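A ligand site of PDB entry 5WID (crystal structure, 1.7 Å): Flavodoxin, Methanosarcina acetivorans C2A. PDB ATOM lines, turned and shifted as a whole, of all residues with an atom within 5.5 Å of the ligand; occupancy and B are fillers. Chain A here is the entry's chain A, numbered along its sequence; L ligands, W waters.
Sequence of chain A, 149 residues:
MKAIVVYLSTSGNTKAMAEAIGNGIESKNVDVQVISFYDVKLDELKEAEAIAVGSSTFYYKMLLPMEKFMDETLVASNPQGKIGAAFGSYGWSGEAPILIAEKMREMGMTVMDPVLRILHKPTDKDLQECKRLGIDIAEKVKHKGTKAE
The backbone NH (N) of Gly 12 lies within hydrogen-bond range of the side-chain hydroxyl (OG) of Ser 9 (3.0 Å). The backbone NH of Ser 56 is in hydrogen-bond range of the side-chain hydroxyl of Thr 14. The backbone carbonyl oxygen (O) of Ile 118 sits close to the side-chain hydroxyl (OG) of Ser 89 (3.2 Å). O of Ile 118 lies within hydrogen-bond range of N of Tyr 90 (3.1 Å). N of Thr 57 lies within hydrogen-bond range of O of Ser 89 (3.5 Å). The side-chain hydroxyl of Ser 9 is in hydrogen-bond range of the backbone NH of Lys 15. The side-chain carboxylate of Glu 95 lies within hydrogen-bond range of the side-chain hydroxyl of Ser 93, at 2.6 Å. The backbone NH (N) of Ser 89 lies within hydrogen-bond range of the side-chain hydroxyl (OG1) of Thr 14, at 3.1 Å.
Water W2 lies within hydrogen-bond range of O4 of the ligand (2.6 Å) and ND1 of His 120 (2.9 Å).
N of Ser 11 sits at hydrogen-bond distance from O9 of the ligand (2.9 Å). The backbone NH of Asn 13 lies within hydrogen-bond range of an oxygen (O9) of the ligand (3.0 Å). N of Gly 94 is in hydrogen-bond range of O1 of the ligand (2.9 Å). OG of Ser 93 sits at hydrogen-bond distance from N2 of the ligand (2.7 Å). An oxygen (O7) of the ligand is in hydrogen-bond range of the side-chain hydroxyl (OG) of Ser 9, at 2.8 Å. N of Gly 12 lies within hydrogen-bond range of O9 of the ligand (3.1 Å). The side-chain amide nitrogen of Asn 13 is in hydrogen-bond range of an oxygen (O5) of the ligand. The side-chain hydroxyl (OG1) of Thr 10 lies within hydrogen-bond range of an oxygen (O8) of the ligand, 2.7 Å away. O3 of the ligand sits at hydrogen-bond distance from O of Thr 57, 2.8 Å away. The backbone NH of Thr 10 lies within hydrogen-bond range of an oxygen (O8) of the ligand, at 2.8 Å. An oxygen (O2) of the ligand sits at hydrogen-bond distance from the backbone NH (N) of Tyr 60 (3.0 Å). N of Ser 93 sits at hydrogen-bond distance from O1 of the ligand, 2.8 Å away. The side-chain hydroxyl (OG) of Ser 89 is in hydrogen-bond range of an oxygen (O5) of the ligand (2.7 Å). OG1 of Thr 14 lies within hydrogen-bond range of O7 of the ligand (2.7 Å). An oxygen (O1) of the ligand lies within hydrogen-bond range of the backbone NH of Trp 92 (2.9 Å). O8 of the ligand sits at hydrogen-bond distance from OG of Ser 56, 2.7 Å away. An oxygen (O7) of the ligand is in hydrogen-bond range of the backbone NH of Thr 14. A nitrogen (N1) of the ligand sits at hydrogen-bond distance from the backbone NH (N) of Gly 91 (3.0 Å). The side-chain hydroxyl of Ser 11 lies within hydrogen-bond range of an oxygen (O9) of the ligand (2.6 Å). The backbone NH of Tyr 59 is in hydrogen-bond range of an oxygen (O2) of the ligand (3.0 Å).
Phe 58 touches the ligand. Tyr 90 touches the ligand. CA of His 120 touches O5 of the ligand, at 3.9 Å. Hydrophobic or aromatic side chains that line the ligand: Phe 58, Tyr 59, Tyr 60, Tyr 90 and Trp 92. Of the 25 residues printed, 18 come within 4 Å of the ligand.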
ATOM      1  N   LEU A   8      14.338 -16.733 -21.036  1.00  0.00           N
ATOM      2  CA  LEU A   8      15.560 -16.283 -20.389  1.00  0.00           C
ATOM      3  C   LEU A   8      15.753 -17.137 -19.153  1.00  0.00           C
ATOM      4  O   LEU A   8      14.817 -17.310 -18.361  1.00  0.00           O
ATOM      5  CB  LEU A   8      15.480 -14.806 -19.991  1.00  0.00           C
ATOM      6  CG  LEU A   8      16.772 -14.200 -19.411  1.00  0.00           C
ATOM      7  CD1 LEU A   8      16.886 -12.705 -19.752  1.00  0.00           C
ATOM      8  CD2 LEU A   8      16.828 -14.392 -17.891  1.00  0.00           C
ATOM      9  N   SER A   9      16.976 -17.623 -18.936  1.00  0.00           N
ATOM     10  CA  SER A   9      17.247 -18.441 -17.764  1.00  0.00           C
ATOM     11  C   SER A   9      18.671 -18.198 -17.288  1.00  0.00           C
ATOM     12  O   SER A   9      19.581 -18.164 -18.118  1.00  0.00           O
ATOM     13  CB  SER A   9      17.039 -19.937 -18.105  1.00  0.00           C
ATOM     14  OG  SER A   9      17.156 -20.737 -16.938  1.00  0.00           O
ATOM     15  N   THR A  10      18.845 -18.025 -15.976  1.00  0.00           N
ATOM     16  CA  THR A  10      20.169 -17.759 -15.408  1.00  0.00           C
ATOM     17  C   THR A  10      20.862 -18.994 -14.851  1.00  0.00           C
ATOM     18  O   THR A  10      22.096 -19.049 -14.801  1.00  0.00           O
ATOM     19  CB  THR A  10      20.090 -16.706 -14.287  1.00  0.00           C
ATOM     20  OG1 THR A  10      19.395 -17.226 -13.155  1.00  0.00           O
ATOM     21  CG2 THR A  10      19.372 -15.434 -14.782  1.00  0.00           C
ATOM     22  N   SER A  11      20.102 -20.003 -14.432  1.00  0.00           N
ATOM     23  CA  SER A  11      20.670 -21.211 -13.872  1.00  0.00           C
ATOM     24  C   SER A  11      20.066 -22.478 -14.449  1.00  0.00           C
ATOM     25  O   SER A  11      20.419 -23.571 -14.016  1.00  0.00           O
ATOM     26  CB  SER A  11      20.522 -21.237 -12.333  1.00  0.00           C
ATOM     27  OG  SER A  11      19.214 -21.633 -11.918  1.00  0.00           O
ATOM     28  N   GLY A  12      19.141 -22.363 -15.417  1.00  0.00           N
ATOM     29  CA  GLY A  12      18.580 -23.513 -16.092  1.00  0.00           C
ATOM     30  C   GLY A  12      17.134 -23.847 -15.734  1.00  0.00           C
ATOM     31  O   GLY A  12      16.536 -24.697 -16.407  1.00  0.00           O
ATOM     32  N   ASN A  13      16.551 -23.206 -14.730  1.00  0.00           N
ATOM     33  CA  ASN A  13      15.232 -23.654 -14.278  1.00  0.00           C
ATOM     34  C   ASN A  13      14.140 -23.269 -15.275  1.00  0.00           C
ATOM     35  O   ASN A  13      13.323 -24.120 -15.664  1.00  0.00           O
ATOM     36  CB  ASN A  13      14.937 -23.092 -12.889  1.00  0.00           C
ATOM     37  CG  ASN A  13      15.844 -23.705 -11.812  1.00  0.00           C
ATOM     38  OD1 ASN A  13      16.332 -24.841 -11.961  1.00  0.00           O
ATOM     39  ND2 ASN A  13      16.073 -22.955 -10.741  1.00  0.00           N
ATOM     40  N   THR A  14      14.107 -22.012 -15.695  1.00  0.00           N
ATOM     41  CA  THR A  14      13.143 -21.603 -16.729  1.00  0.00           C
ATOM     42  C   THR A  14      13.435 -22.299 -18.054  1.00  0.00           C
ATOM     43  O   THR A  14      12.501 -22.618 -18.809  1.00  0.00           O
ATOM     44  CB  THR A  14      13.167 -20.080 -16.880  1.00  0.00           C
ATOM     45  OG1 THR A  14      12.907 -19.502 -15.591  1.00  0.00           O
ATOM     46  CG2 THR A  14      12.108 -19.574 -17.890  1.00  0.00           C
ATOM     47  N   LYS A  15      14.706 -22.563 -18.345  1.00  0.00           N
ATOM     48  CA  LYS A  15      15.023 -23.326 -19.550  1.00  0.00           C
ATOM     49  C   LYS A  15      14.420 -24.722 -19.480  1.00  0.00           C
ATOM     50  O   LYS A  15      13.837 -25.212 -20.464  1.00  0.00           O
ATOM     51  CB  LYS A  15      16.543 -23.422 -19.731  1.00  0.00           C
ATOM     52  CG  LYS A  15      16.986 -24.274 -20.942  1.00  0.00           C
ATOM     53  CD  LYS A  15      18.527 -24.231 -21.093  1.00  0.00           C
ATOM     54  CE  LYS A  15      18.979 -24.958 -22.360  1.00  0.00           C
ATOM     55  NZ  LYS A  15      18.674 -26.422 -22.255  1.00  0.00           N
ATOM     56  N   SER A  56      12.899 -16.033 -15.462  1.00  0.00           N
ATOM     57  CA  SER A  56      12.918 -16.070 -14.017  1.00  0.00           C
ATOM     58  C   SER A  56      12.663 -14.665 -13.467  1.00  0.00           C
ATOM     59  O   SER A  56      12.593 -13.679 -14.203  1.00  0.00           O
ATOM     60  CB  SER A  56      14.241 -16.643 -13.504  1.00  0.00           C
ATOM     61  OG  SER A  56      15.342 -16.006 -14.146  1.00  0.00           O
ATOM     62  N   THR A  57      12.467 -14.588 -12.148  1.00  0.00           N
ATOM     63  CA  THR A  57      12.208 -13.332 -11.455  1.00  0.00           C
ATOM     64  C   THR A  57      13.480 -12.947 -10.702  1.00  0.00           C
ATOM     65  O   THR A  57      13.967 -13.721  -9.879  1.00  0.00           O
ATOM     66  CB  THR A  57      11.047 -13.470 -10.466  1.00  0.00           C
ATOM     67  OG1 THR A  57       9.835 -13.837 -11.148  1.00  0.00           O
ATOM     68  CG2 THR A  57      10.821 -12.147  -9.707  1.00  0.00           C
ATOM     69  N   PHE A  58      14.027 -11.777 -11.017  1.00  0.00           N
ATOM     70  CA  PHE A  58      15.139 -11.195 -10.267  1.00  0.00           C
ATOM     71  C   PHE A  58      14.695  -9.840  -9.752  1.00  0.00           C
ATOM     72  O   PHE A  58      14.298  -8.986 -10.552  1.00  0.00           O
ATOM     73  CB  PHE A  58      16.390 -11.033 -11.133  1.00  0.00           C
ATOM     74  CG  PHE A  58      17.317 -12.222 -11.118  1.00  0.00           C
ATOM     75  CD1 PHE A  58      16.848 -13.505 -11.393  1.00  0.00           C
ATOM     76  CD2 PHE A  58      18.660 -12.047 -10.853  1.00  0.00           C
ATOM     77  CE1 PHE A  58      17.719 -14.594 -11.388  1.00  0.00           C
ATOM     78  CE2 PHE A  58      19.539 -13.126 -10.852  1.00  0.00           C
ATOM     79  CZ  PHE A  58      19.070 -14.389 -11.126  1.00  0.00           C
ATOM     80  N   TYR A  59      14.779  -9.639  -8.434  1.00  0.00           N
ATOM     81  CA  TYR A  59      14.383  -8.391  -7.802  1.00  0.00           C
ATOM     82  C   TYR A  59      13.050  -7.896  -8.360  1.00  0.00           C
ATOM     83  O   TYR A  59      12.922  -6.767  -8.837  1.00  0.00           O
ATOM     84  CB  TYR A  59      15.495  -7.334  -7.935  1.00  0.00           C
ATOM     85  CG  TYR A  59      16.752  -7.825  -7.288  1.00  0.00           C
ATOM     86  CD1 TYR A  59      16.831  -7.958  -5.905  1.00  0.00           C
ATOM     87  CD2 TYR A  59      17.848  -8.233  -8.051  1.00  0.00           C
ATOM     88  CE1 TYR A  59      17.966  -8.459  -5.294  1.00  0.00           C
ATOM     89  CE2 TYR A  59      19.009  -8.724  -7.431  1.00  0.00           C
ATOM     90  CZ  TYR A  59      19.048  -8.837  -6.058  1.00  0.00           C
ATOM     91  OH  TYR A  59      20.166  -9.330  -5.414  1.00  0.00           O
ATOM     92  N   TYR A  60      12.048  -8.778  -8.280  1.00  0.00           N
ATOM     93  CA  TYR A  60      10.624  -8.508  -8.465  1.00  0.00           C
ATOM     94  C   TYR A  60      10.247  -8.205  -9.914  1.00  0.00           C
ATOM     95  O   TYR A  60       9.135  -7.726 -10.160  1.00  0.00           O
ATOM     96  CB  TYR A  60      10.159  -7.369  -7.536  1.00  0.00           C
ATOM     97  CG  TYR A  60      10.841  -7.500  -6.204  1.00  0.00           C
ATOM     98  CD1 TYR A  60      10.563  -8.586  -5.381  1.00  0.00           C
ATOM     99  CD2 TYR A  60      11.815  -6.598  -5.796  1.00  0.00           C
ATOM    100  CE1 TYR A  60      11.212  -8.759  -4.194  1.00  0.00           C
ATOM    101  CE2 TYR A  60      12.477  -6.761  -4.604  1.00  0.00           C
ATOM    102  CZ  TYR A  60      12.167  -7.837  -3.798  1.00  0.00           C
ATOM    103  OH  TYR A  60      12.808  -8.020  -2.605  1.00  0.00           O
ATOM    104  N   LYS A  61      11.127  -8.504 -10.871  1.00  0.00           N
ATOM    105  CA  LYS A  61      10.926  -8.152 -12.266  1.00  0.00           C
ATOM    106  C   LYS A  61      11.399  -9.303 -13.143  1.00  0.00           C
ATOM    107  O   LYS A  61      12.138 -10.181 -12.697  1.00  0.00           O
ATOM    108  CB  LYS A  61      11.713  -6.884 -12.653  1.00  0.00           C
ATOM    109  CG  LYS A  61      11.223  -5.588 -12.000  1.00  0.00           C
ATOM    110  CD  LYS A  61       9.724  -5.408 -12.206  1.00  0.00           C
ATOM    111  CE  LYS A  61       9.206  -4.123 -11.561  1.00  0.00           C
ATOM    112  NZ  LYS A  61       7.779  -3.872 -11.918  1.00  0.00           N
ATOM    113  N   SER A  89      10.460 -19.636 -13.662  1.00  0.00           N
ATOM    114  CA  SER A  89      10.821 -20.152 -12.342  1.00  0.00           C
ATOM    115  C   SER A  89      11.129 -18.981 -11.421  1.00  0.00           C
ATOM    116  O   SER A  89      11.537 -17.906 -11.869  1.00  0.00           O
ATOM    117  CB  SER A  89      12.033 -21.079 -12.451  1.00  0.00           C
ATOM    118  OG  SER A  89      12.467 -21.550 -11.181  1.00  0.00           O
ATOM    119  N   TYR A  90      10.915 -19.174 -10.117  1.00  0.00           N
ATOM    120  CA  TYR A  90      11.095 -18.076  -9.185  1.00  0.00           C
ATOM    121  C   TYR A  90      11.447 -18.625  -7.804  1.00  0.00           C
ATOM    122  O   TYR A  90      11.346 -19.824  -7.557  1.00  0.00           O
ATOM    123  CB  TYR A  90       9.842 -17.188  -9.112  1.00  0.00           C
ATOM    124  CG  TYR A  90       8.665 -17.811  -8.381  1.00  0.00           C
ATOM    125  CD1 TYR A  90       7.933 -18.870  -8.944  1.00  0.00           C
ATOM    126  CD2 TYR A  90       8.262 -17.342  -7.132  1.00  0.00           C
ATOM    127  CE1 TYR A  90       6.845 -19.419  -8.270  1.00  0.00           C
ATOM    128  CE2 TYR A  90       7.170 -17.870  -6.466  1.00  0.00           C
ATOM    129  CZ  TYR A  90       6.468 -18.919  -7.034  1.00  0.00           C
ATOM    130  OH  TYR A  90       5.398 -19.466  -6.370  1.00  0.00           O
ATOM    131  N   GLY A  91      11.835 -17.712  -6.906  1.00  0.00           N
ATOM    132  CA  GLY A  91      12.253 -18.118  -5.578  1.00  0.00           C
ATOM    133  C   GLY A  91      11.300 -17.771  -4.440  1.00  0.00           C
ATOM    134  O   GLY A  91      11.302 -18.483  -3.433  1.00  0.00           O
ATOM    135  N   TRP A  92      10.533 -16.693  -4.549  1.00  0.00           N
ATOM    136  CA  TRP A  92       9.560 -16.422  -3.496  1.00  0.00           C
ATOM    137  C   TRP A  92       8.444 -15.462  -3.910  1.00  0.00           C
ATOM    138  O   TRP A  92       7.299 -15.665  -3.495  1.00  0.00           O
ATOM    139  CB  TRP A  92      10.245 -15.888  -2.222  1.00  0.00           C
ATOM    140  CG  TRP A  92      10.840 -14.512  -2.289  1.00  0.00           C
ATOM    141  CD1 TRP A  92      10.280 -13.346  -1.833  1.00  0.00           C
ATOM    142  CD2 TRP A  92      12.145 -14.152  -2.773  1.00  0.00           C
ATOM    143  NE1 TRP A  92      11.138 -12.289  -2.030  1.00  0.00           N
ATOM    144  CE2 TRP A  92      12.289 -12.758  -2.597  1.00  0.00           C
ATOM    145  CE3 TRP A  92      13.198 -14.883  -3.333  1.00  0.00           C
ATOM    146  CZ2 TRP A  92      13.441 -12.076  -2.978  1.00  0.00           C
ATOM    147  CZ3 TRP A  92      14.355 -14.202  -3.706  1.00  0.00           C
ATOM    148  CH2 TRP A  92      14.463 -12.818  -3.533  1.00  0.00           C
ATOM    149  N   SER A  93       8.761 -14.428  -4.688  1.00  0.00           N
ATOM    150  CA  SER A  93       7.751 -13.430  -5.033  1.00  0.00           C
ATOM    151  C   SER A  93       7.106 -13.677  -6.394  1.00  0.00           C
ATOM    152  O   SER A  93       5.892 -13.497  -6.541  1.00  0.00           O
ATOM    153  CB  SER A  93       8.369 -12.021  -4.973  1.00  0.00           C
ATOM    154  OG  SER A  93       9.353 -11.796  -5.961  1.00  0.00           O
ATOM    155  N   GLY A  94       7.886 -14.066  -7.392  1.00  0.00           N
ATOM    156  CA  GLY A  94       7.321 -14.641  -8.620  1.00  0.00           C
ATOM    157  C   GLY A  94       6.567 -13.705  -9.537  1.00  0.00           C
ATOM    158  O   GLY A  94       5.617 -14.149 -10.209  1.00  0.00           O
ATOM    159  N   GLU A  95       6.991 -12.449  -9.652  1.00  0.00           N
ATOM    160  CA  GLU A  95       6.269 -11.488 -10.470  1.00  0.00           C
ATOM    161  C   GLU A  95       6.494 -11.684 -11.973  1.00  0.00           C
ATOM    162  O   GLU A  95       5.614 -11.309 -12.756  1.00  0.00           O
ATOM    163  CB  GLU A  95       6.666 -10.040 -10.124  1.00  0.00           C
ATOM    164  CG  GLU A  95       6.188  -9.539  -8.761  1.00  0.00           C
ATOM    165  CD  GLU A  95       7.189  -9.812  -7.650  1.00  0.00           C
ATOM    166  OE1 GLU A  95       8.129 -10.617  -7.864  1.00  0.00           O
ATOM    167  OE2 GLU A  95       7.050  -9.240  -6.555  1.00  0.00           O
ATOM    168  N   ILE A 118       6.834 -21.658 -11.320  1.00  0.00           N
ATOM    169  CA  ILE A 118       7.263 -22.830 -10.554  1.00  0.00           C
ATOM    170  C   ILE A 118       8.421 -22.446  -9.657  1.00  0.00           C
ATOM    171  O   ILE A 118       9.428 -21.902 -10.125  1.00  0.00           O
ATOM    172  CB  ILE A 118       7.701 -23.979 -11.492  1.00  0.00           C
ATOM    173  CG1 ILE A 118       6.520 -24.466 -12.335  1.00  0.00           C
ATOM    174  CG2 ILE A 118       8.262 -25.152 -10.674  1.00  0.00           C
ATOM    175  CD1 ILE A 118       5.537 -25.281 -11.539  1.00  0.00           C
ATOM    176  N   LEU A 119       8.312 -22.777  -8.363  1.00  0.00           N
ATOM    177  CA  LEU A 119       9.367 -22.469  -7.412  1.00  0.00           C
ATOM    178  C   LEU A 119      10.620 -23.306  -7.665  1.00  0.00           C
ATOM    179  O   LEU A 119      10.550 -24.530  -7.816  1.00  0.00           O
ATOM    180  CB  LEU A 119       8.869 -22.713  -5.985  1.00  0.00           C
ATOM    181  CG  LEU A 119       8.009 -21.621  -5.377  1.00  0.00           C
ATOM    182  CD1 LEU A 119       7.223 -22.205  -4.208  1.00  0.00           C
ATOM    183  CD2 LEU A 119       8.896 -20.463  -4.918  1.00  0.00           C
ATOM    184  N   HIS A 120      11.779 -22.634  -7.706  1.00  0.00           N
ATOM    185  CA  HIS A 120      13.117 -23.256  -7.686  1.00  0.00           C
ATOM    186  C   HIS A 120      13.251 -24.246  -8.846  1.00  0.00           C
ATOM    187  O   HIS A 120      12.765 -23.985  -9.960  1.00  0.00           O
ATOM    188  CB  HIS A 120      13.370 -23.867  -6.322  1.00  0.00           C
ATOM    189  CG  HIS A 120      13.093 -22.939  -5.176  1.00  0.00           C
ATOM    190  ND1 HIS A 120      13.707 -21.714  -5.056  1.00  0.00           N
ATOM    191  CD2 HIS A 120      12.276 -23.066  -4.105  1.00  0.00           C
ATOM    192  CE1 HIS A 120      13.282 -21.116  -3.959  1.00  0.00           C
ATOM    193  NE2 HIS A 120      12.406 -21.917  -3.360  1.00  0.00           N
ATOM    194  N   LYS A 121      13.922 -25.381  -8.628  1.00  0.00           N
ATOM    195  CA  LYS A 121      14.156 -26.312  -9.727  1.00  0.00           C
ATOM    196  C   LYS A 121      12.916 -27.158  -9.970  1.00  0.00           C
ATOM    197  O   LYS A 121      12.398 -27.775  -9.023  1.00  0.00           O
ATOM    198  CB  LYS A 121      15.334 -27.216  -9.402  1.00  0.00           C
ATOM    199  CG  LYS A 121      15.638 -28.227 -10.486  1.00  0.00           C
ATOM    200  CD  LYS A 121      16.781 -29.139 -10.039  1.00  0.00           C
ATOM    201  CE  LYS A 121      17.028 -30.256 -11.051  1.00  0.00           C
ATOM    202  NZ  LYS A 121      17.669 -29.721 -12.278  1.00  0.00           N
HETATM  203  N1  LIG L   1      12.891 -14.916  -6.985  1.00  0.00           N
HETATM  204  C1  LIG L   1      11.738 -14.206  -6.749  1.00  0.00           C
HETATM  205  O1  LIG L   1      10.658 -14.797  -6.702  1.00  0.00           O
HETATM  206  N2  LIG L   1      11.798 -12.834  -6.561  1.00  0.00           N
HETATM  207  C2  LIG L   1      12.992 -12.161  -6.622  1.00  0.00           C
HETATM  208  O2  LIG L   1      12.986 -10.928  -6.462  1.00  0.00           O
HETATM  209  C3  LIG L   1      14.159 -12.891  -6.856  1.00  0.00           C
HETATM  210  N3  LIG L   1      15.385 -12.258  -6.903  1.00  0.00           N
HETATM  211  C4  LIG L   1      16.534 -12.978  -7.126  1.00  0.00           C
HETATM  212  C5  LIG L   1      17.765 -12.316  -7.162  1.00  0.00           C
HETATM  213  C6  LIG L   1      18.923 -13.026  -7.390  1.00  0.00           C
HETATM  214  C7  LIG L   1      20.229 -12.282  -7.429  1.00  0.00           C
HETATM  215  C8  LIG L   1      18.882 -14.408  -7.565  1.00  0.00           C
HETATM  216  C9  LIG L   1      20.138 -15.196  -7.807  1.00  0.00           C
HETATM  217  C10 LIG L   1      17.651 -15.081  -7.530  1.00  0.00           C
HETATM  218  C11 LIG L   1      16.479 -14.361  -7.305  1.00  0.00           C
HETATM  219  N4  LIG L   1      15.257 -15.003  -7.273  1.00  0.00           N
HETATM  220  C12 LIG L   1      14.104 -14.273  -7.035  1.00  0.00           C
HETATM  221  C13 LIG L   1      15.168 -16.487  -7.438  1.00  0.00           C
HETATM  222  C14 LIG L   1      15.172 -16.960  -8.889  1.00  0.00           C
HETATM  223  O3  LIG L   1      14.068 -16.470  -9.632  1.00  0.00           O
HETATM  224  C15 LIG L   1      15.113 -18.486  -8.843  1.00  0.00           C
HETATM  225  O4  LIG L   1      16.332 -18.970  -8.325  1.00  0.00           O
HETATM  226  C16 LIG L   1      14.811 -19.140 -10.201  1.00  0.00           C
HETATM  227  O5  LIG L   1      14.632 -20.519  -9.966  1.00  0.00           O
HETATM  228  C17 LIG L   1      15.905 -18.919 -11.239  1.00  0.00           C
HETATM  229  O6  LIG L   1      15.447 -19.493 -12.459  1.00  0.00           O
HETATM  230  P1  LIG L   1      16.400 -19.520 -13.752  1.00  0.00           P
HETATM  231  O7  LIG L   1      15.509 -19.823 -14.921  1.00  0.00           O
HETATM  232  O8  LIG L   1      17.021 -18.138 -13.914  1.00  0.00           O
HETATM  233  O9  LIG L   1      17.449 -20.579 -13.547  1.00  0.00           O
HETATM  234  O   HOH W   1      19.052 -18.751  -8.772  1.00  0.00           O
HETATM  235  O   HOH W   2      16.033 -20.989  -6.678  1.00  0.00           O
